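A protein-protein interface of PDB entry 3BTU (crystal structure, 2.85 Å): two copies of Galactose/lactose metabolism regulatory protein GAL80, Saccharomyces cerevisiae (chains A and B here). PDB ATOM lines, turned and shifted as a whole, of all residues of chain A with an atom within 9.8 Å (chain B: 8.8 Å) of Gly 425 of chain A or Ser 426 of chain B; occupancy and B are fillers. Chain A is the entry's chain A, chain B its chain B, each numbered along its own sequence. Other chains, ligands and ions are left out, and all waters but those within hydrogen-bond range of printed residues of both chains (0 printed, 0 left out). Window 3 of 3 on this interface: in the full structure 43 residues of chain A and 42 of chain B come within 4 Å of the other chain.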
ATOM      1  N   ARG A 231       0.245   2.799 -21.164  1.00  0.00           N
ATOM      2  CA  ARG A 231       0.805   3.766 -22.105  1.00  0.00           C
ATOM      3  C   ARG A 231       1.239   3.001 -23.344  1.00  0.00           C
ATOM      4  O   ARG A 231       1.650   1.849 -23.236  1.00  0.00           O
ATOM      5  CB  ARG A 231       2.008   4.494 -21.497  1.00  0.00           C
ATOM      6  CG  ARG A 231       1.712   5.229 -20.193  1.00  0.00           C
ATOM      7  CD  ARG A 231       2.978   5.788 -19.525  1.00  0.00           C
ATOM      8  NE  ARG A 231       3.531   6.945 -20.228  1.00  0.00           N
ATOM      9  CZ  ARG A 231       3.048   8.182 -20.130  1.00  0.00           C
ATOM     10  NH1 ARG A 231       1.992   8.415 -19.357  1.00  0.00           N
ATOM     11  NH2 ARG A 231       3.613   9.179 -20.807  1.00  0.00           N
ATOM     12  N   ILE A 232       1.139   3.611 -24.521  1.00  0.00           N
ATOM     13  CA  ILE A 232       1.687   2.966 -25.708  1.00  0.00           C
ATOM     14  C   ILE A 232       2.351   3.971 -26.617  1.00  0.00           C
ATOM     15  O   ILE A 232       2.080   5.164 -26.524  1.00  0.00           O
ATOM     16  CB  ILE A 232       0.603   2.249 -26.528  1.00  0.00           C
ATOM     17  CG1 ILE A 232       0.011   3.215 -27.558  1.00  0.00           C
ATOM     18  CG2 ILE A 232      -0.459   1.653 -25.610  1.00  0.00           C
ATOM     19  CD1 ILE A 232      -1.434   2.971 -27.856  1.00  0.00           C
ATOM     20  N   ASN A 233       3.223   3.481 -27.492  1.00  0.00           N
ATOM     21  CA  ASN A 233       3.771   4.298 -28.561  1.00  0.00           C
ATOM     22  C   ASN A 233       4.035   3.490 -29.818  1.00  0.00           C
ATOM     23  O   ASN A 233       4.709   2.458 -29.767  1.00  0.00           O
ATOM     24  CB  ASN A 233       5.054   4.995 -28.137  1.00  0.00           C
ATOM     25  CG  ASN A 233       5.736   5.688 -29.301  1.00  0.00           C
ATOM     26  OD1 ASN A 233       6.312   5.036 -30.170  1.00  0.00           O
ATOM     27  ND2 ASN A 233       5.661   7.016 -29.331  1.00  0.00           N
ATOM     28  N   ALA A 234       3.528   3.967 -30.951  1.00  0.00           N
ATOM     29  CA  ALA A 234       3.666   3.220 -32.196  1.00  0.00           C
ATOM     30  C   ALA A 234       4.320   4.016 -33.322  1.00  0.00           C
ATOM     31  O   ALA A 234       4.322   5.245 -33.317  1.00  0.00           O
ATOM     32  CB  ALA A 234       2.296   2.688 -32.647  1.00  0.00           C
ATOM     33  N   MET A 235       4.878   3.300 -34.288  1.00  0.00           N
ATOM     34  CA  MET A 235       5.308   3.899 -35.547  1.00  0.00           C
ATOM     35  C   MET A 235       4.806   3.030 -36.691  1.00  0.00           C
ATOM     36  O   MET A 235       5.074   1.828 -36.716  1.00  0.00           O
ATOM     37  CB  MET A 235       6.828   4.028 -35.617  1.00  0.00           C
ATOM     38  CG  MET A 235       7.443   4.776 -34.457  1.00  0.00           C
ATOM     39  SD  MET A 235       9.223   5.010 -34.675  1.00  0.00           S
ATOM     40  CE  MET A 235       9.609   5.900 -33.179  1.00  0.00           C
ATOM     41  N   VAL A 236       4.078   3.639 -37.626  1.00  0.00           N
ATOM     42  CA  VAL A 236       3.469   2.902 -38.740  1.00  0.00           C
ATOM     43  C   VAL A 236       4.122   3.232 -40.087  1.00  0.00           C
ATOM     44  O   VAL A 236       4.222   4.400 -40.451  1.00  0.00           O
ATOM     45  CB  VAL A 236       1.980   3.186 -38.809  1.00  0.00           C
ATOM     46  CG1 VAL A 236       1.361   2.446 -39.976  1.00  0.00           C
ATOM     47  CG2 VAL A 236       1.324   2.788 -37.499  1.00  0.00           C
ATOM     48  N   GLN A 268       4.696  -0.669 -28.876  1.00  0.00           N
ATOM     49  CA  GLN A 268       5.544  -0.611 -27.696  1.00  0.00           C
ATOM     50  C   GLN A 268       4.780   0.049 -26.572  1.00  0.00           C
ATOM     51  O   GLN A 268       4.354   1.193 -26.705  1.00  0.00           O
ATOM     52  CB  GLN A 268       6.764   0.235 -28.042  1.00  0.00           C
ATOM     53  CG  GLN A 268       7.834   0.305 -26.993  1.00  0.00           C
ATOM     54  CD  GLN A 268       9.035   1.099 -27.480  1.00  0.00           C
ATOM     55  OE1 GLN A 268       8.964   2.318 -27.638  1.00  0.00           O
ATOM     56  NE2 GLN A 268      10.147   0.408 -27.722  1.00  0.00           N
ATOM     57  N   SER A 417      -5.822   4.369 -31.239  1.00  0.00           N
ATOM     58  CA  SER A 417      -4.722   4.925 -30.472  1.00  0.00           C
ATOM     59  C   SER A 417      -3.388   4.666 -31.147  1.00  0.00           C
ATOM     60  O   SER A 417      -2.529   5.551 -31.185  1.00  0.00           O
ATOM     61  CB  SER A 417      -4.724   4.365 -29.061  1.00  0.00           C
ATOM     62  OG  SER A 417      -5.848   4.864 -28.367  1.00  0.00           O
ATOM     63  N   VAL A 418      -3.219   3.470 -31.695  1.00  0.00           N
ATOM     64  CA  VAL A 418      -1.979   3.140 -32.383  1.00  0.00           C
ATOM     65  C   VAL A 418      -1.723   4.051 -33.578  1.00  0.00           C
ATOM     66  O   VAL A 418      -0.602   4.498 -33.793  1.00  0.00           O
ATOM     67  CB  VAL A 418      -1.947   1.666 -32.839  1.00  0.00           C
ATOM     68  CG1 VAL A 418      -0.647   1.363 -33.582  1.00  0.00           C
ATOM     69  CG2 VAL A 418      -2.098   0.732 -31.634  1.00  0.00           C
ATOM     70  N   TYR A 419      -2.760   4.332 -34.354  1.00  0.00           N
ATOM     71  CA  TYR A 419      -2.616   5.230 -35.493  1.00  0.00           C
ATOM     72  C   TYR A 419      -2.446   6.666 -35.041  1.00  0.00           C
ATOM     73  O   TYR A 419      -1.605   7.394 -35.555  1.00  0.00           O
ATOM     74  CB  TYR A 419      -3.835   5.127 -36.405  1.00  0.00           C
ATOM     75  CG  TYR A 419      -3.764   3.995 -37.386  1.00  0.00           C
ATOM     76  CD1 TYR A 419      -4.471   2.821 -37.170  1.00  0.00           C
ATOM     77  CD2 TYR A 419      -2.980   4.098 -38.527  1.00  0.00           C
ATOM     78  CE1 TYR A 419      -4.407   1.778 -38.065  1.00  0.00           C
ATOM     79  CE2 TYR A 419      -2.901   3.060 -39.431  1.00  0.00           C
ATOM     80  CZ  TYR A 419      -3.619   1.900 -39.199  1.00  0.00           C
ATOM     81  OH  TYR A 419      -3.551   0.858 -40.102  1.00  0.00           O
ATOM     82  N   LYS A 420      -3.268   7.063 -34.081  1.00  0.00           N
ATOM     83  CA  LYS A 420      -3.229   8.409 -33.537  1.00  0.00           C
ATOM     84  C   LYS A 420      -1.834   8.684 -32.996  1.00  0.00           C
ATOM     85  O   LYS A 420      -1.273   9.755 -33.213  1.00  0.00           O
ATOM     86  CB  LYS A 420      -4.279   8.555 -32.431  1.00  0.00           C
ATOM     87  CG  LYS A 420      -5.079   9.853 -32.473  1.00  0.00           C
ATOM     88  CD  LYS A 420      -4.732  10.779 -31.302  1.00  0.00           C
ATOM     89  CE  LYS A 420      -5.460  12.128 -31.413  1.00  0.00           C
ATOM     90  NZ  LYS A 420      -6.897  11.996 -31.799  1.00  0.00           N
ATOM     91  N   SER A 421      -1.272   7.701 -32.306  1.00  0.00           N
ATOM     92  CA  SER A 421       0.064   7.831 -31.745  1.00  0.00           C
ATOM     93  C   SER A 421       1.117   8.028 -32.823  1.00  0.00           C
ATOM     94  O   SER A 421       2.037   8.828 -32.672  1.00  0.00           O
ATOM     95  CB  SER A 421       0.417   6.600 -30.916  1.00  0.00           C
ATOM     96  OG  SER A 421       1.779   6.634 -30.506  1.00  0.00           O
ATOM     97  N   ASN A 422       0.996   7.273 -33.905  1.00  0.00           N
ATOM     98  CA  ASN A 422       1.923   7.405 -35.023  1.00  0.00           C
ATOM     99  C   ASN A 422       1.904   8.810 -35.637  1.00  0.00           C
ATOM    100  O   ASN A 422       2.958   9.389 -35.900  1.00  0.00           O
ATOM    101  CB  ASN A 422       1.625   6.348 -36.092  1.00  0.00           C
ATOM    102  CG  ASN A 422       2.544   6.460 -37.293  1.00  0.00           C
ATOM    103  OD1 ASN A 422       3.723   6.093 -37.231  1.00  0.00           O
ATOM    104  ND2 ASN A 422       2.007   6.973 -38.399  1.00  0.00           N
ATOM    105  N   MET A 423       0.701   9.339 -35.860  1.00  0.00           N
ATOM    106  CA  MET A 423       0.511  10.662 -36.453  1.00  0.00           C
ATOM    107  C   MET A 423       1.121  11.752 -35.588  1.00  0.00           C
ATOM    108  O   MET A 423       1.914  12.572 -36.049  1.00  0.00           O
ATOM    109  CB  MET A 423      -0.983  10.964 -36.621  1.00  0.00           C
ATOM    110  CG  MET A 423      -1.668  10.282 -37.798  1.00  0.00           C
ATOM    111  SD  MET A 423      -1.307  11.045 -39.395  1.00  0.00           S
ATOM    112  CE  MET A 423       0.220  10.223 -39.863  1.00  0.00           C
ATOM    113  N   MET A 424       0.723  11.754 -34.325  1.00  0.00           N
ATOM    114  CA  MET A 424       1.142  12.769 -33.383  1.00  0.00           C
ATOM    115  C   MET A 424       2.585  12.580 -32.971  1.00  0.00           C
ATOM    116  O   MET A 424       3.249  13.530 -32.560  1.00  0.00           O
ATOM    117  CB  MET A 424       0.247  12.715 -32.151  1.00  0.00           C
ATOM    118  CG  MET A 424      -1.232  12.745 -32.486  1.00  0.00           C
ATOM    119  SD  MET A 424      -2.204  13.272 -31.073  1.00  0.00           S
ATOM    120  CE  MET A 424      -1.524  12.214 -29.806  1.00  0.00           C
ATOM    121  N   GLY A 425       3.071  11.348 -33.083  1.00  0.00           N
ATOM    122  CA  GLY A 425       4.429  11.030 -32.695  1.00  0.00           C
ATOM    123  C   GLY A 425       4.624  11.213 -31.205  1.00  0.00           C
ATOM    124  O   GLY A 425       5.606  11.808 -30.766  1.00  0.00           O
ATOM    125  N   SER A 426       3.684  10.702 -30.419  1.00  0.00           N
ATOM    126  CA  SER A 426       3.822  10.752 -28.977  1.00  0.00           C
ATOM    127  C   SER A 426       3.240   9.526 -28.289  1.00  0.00           C
ATOM    128  O   SER A 426       2.236   8.958 -28.731  1.00  0.00           O
ATOM    129  CB  SER A 426       3.153  12.005 -28.431  1.00  0.00           C
ATOM    130  OG  SER A 426       1.751  11.811 -28.310  1.00  0.00           O
ATOM    131  N   THR A 427       3.883   9.122 -27.201  1.00  0.00           N
ATOM    132  CA  THR A 427       3.327   8.094 -26.340  1.00  0.00           C
ATOM    133  C   THR A 427       1.959   8.574 -25.850  1.00  0.00           C
ATOM    134  O   THR A 427       1.776   9.766 -25.580  1.00  0.00           O
ATOM    135  CB  THR A 427       4.253   7.827 -25.143  1.00  0.00           C
ATOM    136  OG1 THR A 427       5.555   7.467 -25.618  1.00  0.00           O
ATOM    137  CG2 THR A 427       3.709   6.707 -24.280  1.00  0.00           C
ATOM    138  N   LEU A 428       1.001   7.656 -25.740  1.00  0.00           N
ATOM    139  CA  LEU A 428      -0.359   8.016 -25.347  1.00  0.00           C
ATOM    140  C   LEU A 428      -0.828   7.252 -24.123  1.00  0.00           C
ATOM    141  O   LEU A 428      -0.734   6.033 -24.084  1.00  0.00           O
ATOM    142  CB  LEU A 428      -1.329   7.719 -26.485  1.00  0.00           C
ATOM    143  CG  LEU A 428      -1.141   8.546 -27.750  1.00  0.00           C
ATOM    144  CD1 LEU A 428      -2.147   8.134 -28.815  1.00  0.00           C
ATOM    145  CD2 LEU A 428      -1.280  10.016 -27.415  1.00  0.00           C
ATOM    146  N   ARG B 231      14.134   8.991 -36.312  1.00  0.00           N
ATOM    147  CA  ARG B 231      13.195   9.240 -35.227  1.00  0.00           C
ATOM    148  C   ARG B 231      13.354   8.120 -34.211  1.00  0.00           C
ATOM    149  O   ARG B 231      13.718   7.005 -34.575  1.00  0.00           O
ATOM    150  CB  ARG B 231      11.760   9.263 -35.757  1.00  0.00           C
ATOM    151  CG  ARG B 231      11.507  10.275 -36.870  1.00  0.00           C
ATOM    152  CD  ARG B 231      10.098  10.131 -37.476  1.00  0.00           C
ATOM    153  NE  ARG B 231       9.038  10.604 -36.581  1.00  0.00           N
ATOM    154  CZ  ARG B 231       8.734  11.887 -36.387  1.00  0.00           C
ATOM    155  NH1 ARG B 231       9.410  12.843 -37.022  1.00  0.00           N
ATOM    156  NH2 ARG B 231       7.755  12.216 -35.550  1.00  0.00           N
ATOM    157  N   ILE B 232      13.113   8.395 -32.937  1.00  0.00           N
ATOM    158  CA  ILE B 232      13.131   7.320 -31.954  1.00  0.00           C
ATOM    159  C   ILE B 232      12.088   7.561 -30.889  1.00  0.00           C
ATOM    160  O   ILE B 232      11.656   8.695 -30.684  1.00  0.00           O
ATOM    161  CB  ILE B 232      14.486   7.227 -31.225  1.00  0.00           C
ATOM    162  CG1 ILE B 232      14.482   8.142 -29.998  1.00  0.00           C
ATOM    163  CG2 ILE B 232      15.640   7.558 -32.164  1.00  0.00           C
ATOM    164  CD1 ILE B 232      15.843   8.639 -29.632  1.00  0.00           C
ATOM    165  N   ASN B 233      11.696   6.504 -30.194  1.00  0.00           N
ATOM    166  CA  ASN B 233      10.863   6.653 -29.012  1.00  0.00           C
ATOM    167  C   ASN B 233      11.180   5.588 -27.973  1.00  0.00           C
ATOM    168  O   ASN B 233      11.202   4.389 -28.285  1.00  0.00           O
ATOM    169  CB  ASN B 233       9.384   6.591 -29.374  1.00  0.00           C
ATOM    170  CG  ASN B 233       8.495   6.503 -28.151  1.00  0.00           C
ATOM    171  OD1 ASN B 233       8.420   5.463 -27.490  1.00  0.00           O
ATOM    172  ND2 ASN B 233       7.823   7.600 -27.837  1.00  0.00           N
ATOM    173  N   ALA B 234      11.404   6.009 -26.733  1.00  0.00           N
ATOM    174  CA  ALA B 234      11.803   5.056 -25.702  1.00  0.00           C
ATOM    175  C   ALA B 234      10.895   5.079 -24.486  1.00  0.00           C
ATOM    176  O   ALA B 234      10.192   6.055 -24.233  1.00  0.00           O
ATOM    177  CB  ALA B 234      13.240   5.302 -25.289  1.00  0.00           C
ATOM    178  N   MET B 235      10.921   3.989 -23.732  1.00  0.00           N
ATOM    179  CA  MET B 235      10.301   3.956 -22.419  1.00  0.00           C
ATOM    180  C   MET B 235      11.294   3.307 -21.446  1.00  0.00           C
ATOM    181  O   MET B 235      11.787   2.195 -21.690  1.00  0.00           O
ATOM    182  CB  MET B 235       8.988   3.171 -22.456  1.00  0.00           C
ATOM    183  CG  MET B 235       8.000   3.677 -23.477  1.00  0.00           C
ATOM    184  SD  MET B 235       6.414   2.851 -23.288  1.00  0.00           S
ATOM    185  CE  MET B 235       5.451   3.596 -24.604  1.00  0.00           C
ATOM    186  N   GLN B 268      12.936   2.098 -29.789  1.00  0.00           N
ATOM    187  CA  GLN B 268      12.133   1.913 -30.986  1.00  0.00           C
ATOM    188  C   GLN B 268      12.330   3.108 -31.895  1.00  0.00           C
ATOM    189  O   GLN B 268      12.064   4.233 -31.495  1.00  0.00           O
ATOM    190  CB  GLN B 268      10.675   1.827 -30.557  1.00  0.00           C
ATOM    191  CG  GLN B 268       9.709   1.461 -31.632  1.00  0.00           C
ATOM    192  CD  GLN B 268       8.298   1.346 -31.094  1.00  0.00           C
ATOM    193  OE1 GLN B 268       7.707   2.340 -30.679  1.00  0.00           O
ATOM    194  NE2 GLN B 268       7.744   0.128 -31.104  1.00  0.00           N
ATOM    195  N   SER B 417      18.870  11.528 -25.754  1.00  0.00           N
ATOM    196  CA  SER B 417      17.592  11.526 -26.461  1.00  0.00           C
ATOM    197  C   SER B 417      16.686  10.434 -25.928  1.00  0.00           C
ATOM    198  O   SER B 417      15.494  10.640 -25.741  1.00  0.00           O
ATOM    199  CB  SER B 417      17.801  11.362 -27.965  1.00  0.00           C
ATOM    200  OG  SER B 417      18.395  12.526 -28.519  1.00  0.00           O
ATOM    201  N   VAL B 418      17.260   9.274 -25.661  1.00  0.00           N
ATOM    202  CA  VAL B 418      16.466   8.169 -25.147  1.00  0.00           C
ATOM    203  C   VAL B 418      15.826   8.508 -23.803  1.00  0.00           C
ATOM    204  O   VAL B 418      14.670   8.206 -23.568  1.00  0.00           O
ATOM    205  CB  VAL B 418      17.281   6.874 -25.036  1.00  0.00           C
ATOM    206  CG1 VAL B 418      16.412   5.777 -24.460  1.00  0.00           C
ATOM    207  CG2 VAL B 418      17.832   6.477 -26.405  1.00  0.00           C
ATOM    208  N   TYR B 419      16.572   9.151 -22.921  1.00  0.00           N
ATOM    209  CA  TYR B 419      16.019   9.556 -21.628  1.00  0.00           C
ATOM    210  C   TYR B 419      15.024  10.702 -21.790  1.00  0.00           C
ATOM    211  O   TYR B 419      13.946  10.698 -21.194  1.00  0.00           O
ATOM    212  CB  TYR B 419      17.134   9.971 -20.667  1.00  0.00           C
ATOM    213  CG  TYR B 419      17.776   8.812 -19.955  1.00  0.00           C
ATOM    214  CD1 TYR B 419      19.030   8.337 -20.342  1.00  0.00           C
ATOM    215  CD2 TYR B 419      17.129   8.190 -18.894  1.00  0.00           C
ATOM    216  CE1 TYR B 419      19.614   7.290 -19.688  1.00  0.00           C
ATOM    217  CE2 TYR B 419      17.710   7.130 -18.239  1.00  0.00           C
ATOM    218  CZ  TYR B 419      18.950   6.686 -18.639  1.00  0.00           C
ATOM    219  OH  TYR B 419      19.525   5.619 -17.984  1.00  0.00           O
ATOM    220  N   LYS B 420      15.414  11.689 -22.590  1.00  0.00           N
ATOM    221  CA  LYS B 420      14.584  12.850 -22.858  1.00  0.00           C
ATOM    222  C   LYS B 420      13.247  12.390 -23.423  1.00  0.00           C
ATOM    223  O   LYS B 420      12.193  12.895 -23.040  1.00  0.00           O
ATOM    224  CB  LYS B 420      15.285  13.770 -23.853  1.00  0.00           C
ATOM    225  CG  LYS B 420      15.201  15.249 -23.497  1.00  0.00           C
ATOM    226  CD  LYS B 420      14.349  16.044 -24.462  1.00  0.00           C
ATOM    227  CE  LYS B 420      14.202  17.496 -23.998  1.00  0.00           C
ATOM    228  NZ  LYS B 420      15.492  18.116 -23.558  1.00  0.00           N
ATOM    229  N   SER B 421      13.299  11.415 -24.327  1.00  0.00           N
ATOM    230  CA  SER B 421      12.101  10.880 -24.951  1.00  0.00           C
ATOM    231  C   SER B 421      11.190  10.212 -23.930  1.00  0.00           C
ATOM    232  O   SER B 421       9.977  10.383 -23.964  1.00  0.00           O
ATOM    233  CB  SER B 421      12.486   9.883 -26.030  1.00  0.00           C
ATOM    234  OG  SER B 421      11.342   9.204 -26.510  1.00  0.00           O
ATOM    235  N   ASN B 422      11.779   9.441 -23.025  1.00  0.00           N
ATOM    236  CA  ASN B 422      11.019   8.802 -21.958  1.00  0.00           C
ATOM    237  C   ASN B 422      10.285   9.812 -21.077  1.00  0.00           C
ATOM    238  O   ASN B 422       9.106   9.624 -20.775  1.00  0.00           O
ATOM    239  CB  ASN B 422      11.930   7.924 -21.092  1.00  0.00           C
ATOM    240  CG  ASN B 422      11.174   7.223 -19.977  1.00  0.00           C
ATOM    241  OD1 ASN B 422      10.389   6.295 -20.224  1.00  0.00           O
ATOM    242  ND2 ASN B 422      11.400   7.658 -18.747  1.00  0.00           N
ATOM    243  N   MET B 423      10.992  10.865 -20.662  1.00  0.00           N
ATOM    244  CA  MET B 423      10.434  11.901 -19.790  1.00  0.00           C
ATOM    245  C   MET B 423       9.259  12.600 -20.446  1.00  0.00           C
ATOM    246  O   MET B 423       8.170  12.690 -19.880  1.00  0.00           O
ATOM    247  CB  MET B 423      11.492  12.958 -19.462  1.00  0.00           C
ATOM    248  CG  MET B 423      12.490  12.564 -18.393  1.00  0.00           C
ATOM    249  SD  MET B 423      11.820  12.642 -16.716  1.00  0.00           S
ATOM    250  CE  MET B 423      11.110  11.003 -16.525  1.00  0.00           C
ATOM    251  N   MET B 424       9.505  13.110 -21.645  1.00  0.00           N
ATOM    252  CA  MET B 424       8.514  13.865 -22.387  1.00  0.00           C
ATOM    253  C   MET B 424       7.419  12.963 -22.938  1.00  0.00           C
ATOM    254  O   MET B 424       6.307  13.417 -23.205  1.00  0.00           O
ATOM    255  CB  MET B 424       9.189  14.611 -23.531  1.00  0.00           C
ATOM    256  CG  MET B 424      10.411  15.385 -23.109  1.00  0.00           C
ATOM    257  SD  MET B 424      10.827  16.652 -24.315  1.00  0.00           S
ATOM    258  CE  MET B 424      10.782  15.710 -25.829  1.00  0.00           C
ATOM    259  N   GLY B 425       7.736  11.685 -23.106  1.00  0.00           N
ATOM    260  CA  GLY B 425       6.785  10.737 -23.644  1.00  0.00           C
ATOM    261  C   GLY B 425       6.425  11.076 -25.078  1.00  0.00           C
ATOM    262  O   GLY B 425       5.250  11.069 -25.457  1.00  0.00           O
ATOM    263  N   SER B 426       7.434  11.384 -25.885  1.00  0.00           N
ATOM    264  CA  SER B 426       7.186  11.661 -27.289  1.00  0.00           C
ATOM    265  C   SER B 426       8.309  11.164 -28.186  1.00  0.00           C
ATOM    266  O   SER B 426       9.481  11.189 -27.813  1.00  0.00           O
ATOM    267  CB  SER B 426       6.985  13.156 -27.507  1.00  0.00           C
ATOM    268  OG  SER B 426       8.232  13.817 -27.570  1.00  0.00           O
ATOM    269  N   THR B 427       7.941  10.707 -29.376  1.00  0.00           N
ATOM    270  CA  THR B 427       8.925  10.370 -30.393  1.00  0.00           C
ATOM    271  C   THR B 427       9.750  11.620 -30.684  1.00  0.00           C
ATOM    272  O   THR B 427       9.206  12.720 -30.706  1.00  0.00           O
ATOM    273  CB  THR B 427       8.235   9.881 -31.673  1.00  0.00           C
ATOM    274  OG1 THR B 427       7.425   8.746 -31.356  1.00  0.00           O
ATOM    275  CG2 THR B 427       9.255   9.473 -32.709  1.00  0.00           C
ATOM    276  N   LEU B 428      11.056  11.465 -30.888  1.00  0.00           N
ATOM    277  CA  LEU B 428      11.936  12.615 -31.114  1.00  0.00           C
ATOM    278  C   LEU B 428      12.676  12.525 -32.431  1.00  0.00           C
ATOM    279  O   LEU B 428      13.283  11.500 -32.729  1.00  0.00           O
ATOM    280  CB  LEU B 428      12.978  12.709 -30.004  1.00  0.00           C
ATOM    281  CG  LEU B 428      12.424  12.969 -28.611  1.00  0.00           C
ATOM    282  CD1 LEU B 428      13.541  13.004 -27.592  1.00  0.00           C
ATOM    283  CD2 LEU B 428      11.669  14.265 -28.620  1.00  0.00           C
ATOM    284  N   ASN B 429      12.660  13.588 -33.219  1.00  0.00           N
ATOM    285  CA  ASN B 429      13.503  13.593 -34.401  1.00  0.00           C
ATOM    286  C   ASN B 429      14.941  13.806 -33.964  1.00  0.00           C
ATOM    287  O   ASN B 429      15.232  14.700 -33.176  1.00  0.00           O
ATOM    288  CB  ASN B 429      13.069  14.655 -35.406  1.00  0.00           C
ATOM    289  CG  ASN B 429      13.844  14.574 -36.700  1.00  0.00           C
ATOM    290  OD1 ASN B 429      15.071  14.473 -36.690  1.00  0.00           O
ATOM    291  ND2 ASN B 429      13.133  14.611 -37.824  1.00  0.00           N
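N of Thr 427 of chain A sits at hydrogen-bond distance from O of Gly 425 of chain B (2.9 Å). OE1 of Gln 268 of chain A sits close to OE1 of Gln 268 of chain B, 3.3 Å away. The side-chain amide oxygen (OD1) of Asn 233 of chain A lies close to the side-chain amide oxygen (OE1) of Gln 268 of chain B. ND2 of Asn 233 of chain A lies close to ND2 of Asn 233 of chain B, at 2.7 Å. ND2 of Asn 233 of chain A lies within hydrogen-bond range of OG1 of Thr 427 of chain B. The side-chain amide oxygen (OE1) of Gln 268 of chain A sits close to the backbone carbonyl oxygen (O) of Asn 233 of chain B, 3.1 Å away. N of Thr 427 of chain B is in hydrogen-bond range of O of Gly 425 of chain A. The side-chain amide nitrogen (ND2) of Asn 233 of chain B lies within hydrogen-bond range of the side-chain hydroxyl (OG1) of Thr 427 of chain A (3.2 Å).
The side-chain amide nitrogen of Asn 233 of chain B sits close to the backbone NH of Thr 427 of chain B (3.5 Å). N of Leu 428 of chain B is in hydrogen-bond range of O of Ile 232 of chain B (2.8 Å). The side-chain hydroxyl (OG) of Ser 421 of chain B sits at hydrogen-bond distance from the backbone carbonyl oxygen (O) of Ser 426 of chain B (3.0 Å). The side-chain amide nitrogen (ND2) of Asn 233 of chain A lies close to the backbone NH (N) of Thr 427 of chain A (3.5 Å). N of Asn 233 of chain A lies within hydrogen-bond range of O of Gln 268 of chain A (2.7 Å). The backbone carbonyl oxygen (O) of Gln 268 of chain B sits at hydrogen-bond distance from the backbone NH (N) of Asn 233 of chain B.
Among the printed residues, pairs that only touch across the chains: Gln 268 of chain A with Met 235 of chain B, Met 235 of chain A with Gln 268 of chain B, Thr 427 of chain A with Met 235 of chain B, Met 235 of chain A with Thr 427 of chain B, Asn 233 of chain A with Met 235 of chain B, Met 235 of chain A with Asn 233 of chain B, Ile 232 of chain A with Met 235 of chain B, Ser 426 of chain A with Gly 425 of chain B, Met 235 of chain A with Ile 232 of chain B, Gly 425 of chain A with Ser 426 of chain B and Ser 426 of chain A with Ser 426 of chain B.
Printed residues of chain B within 4 Å of Asn 233 of chain A: Asn 233, Met 235, Gln 268 and Thr 427. Printed residues of chain B within 4 Å of Gln 268 of chain A: Asn 233, Met 235 and Gln 268. Gly 425 of chain A touches two residues of chain B. Ser 426 of chain A touches just these residues of chain B: Gly 425 (3.8 Å) and Ser 426 (3.9 Å). Tyr 419 of chain B touches none of the printed residues of chain A. No residue of chain A comes within 4 Å of Ser 421 of chain B. Met 424 of chain B touches none of the printed residues of chain A. Of chain A, only Ser 426 (3.8 Å) and Thr 427 (2.9 Å) come within 4 Å of Gly 425 of chain B. Ser 426 of chain B touches just these residues of chain A: Gly 425 (3.8 Å) and Ser 426 (3.9 Å). The nearest printed residue of chain B that does not touch Thr 427 of chain A is Ser 426 of chain B (4.2 Å).
Of the 19 printed residues of chain A, 7 touch a printed residue of chain B. Hydrophobic or aromatic side chains of chain A that line the printed part of chain B: Met 235. Hydrophobic or aromatic side chains of chain B within 4 Å of the printed part of chain A: Met 235. Among the printed residues, no Asp or Glu carboxylate lies within 4 Å of a Lys or Arg side-chain nitrogen of the other chain.
Asn 233 of chain A touches Thr 427 of chain B, and with the chains exchanged Thr 427 of chain A touches Asn 233 of chain B. Met 235 of chain A touches Gln 268 of chain B, and with the chains exchanged Gln 268 of chain A touches Met 235 of chain B. Gly 425 of chain A touches Ser 426 of chain B, and with the chains exchanged Ser 426 of chain A touches Gly 425 of chain B. Ser 426 of chain A touches its own counterpart, Ser 426 of chain B. 18 positions are printed for both chains. Of the 19 pairs that touch across the chains among the printed residues, 19 have their exchanged pair printed and touching as well.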
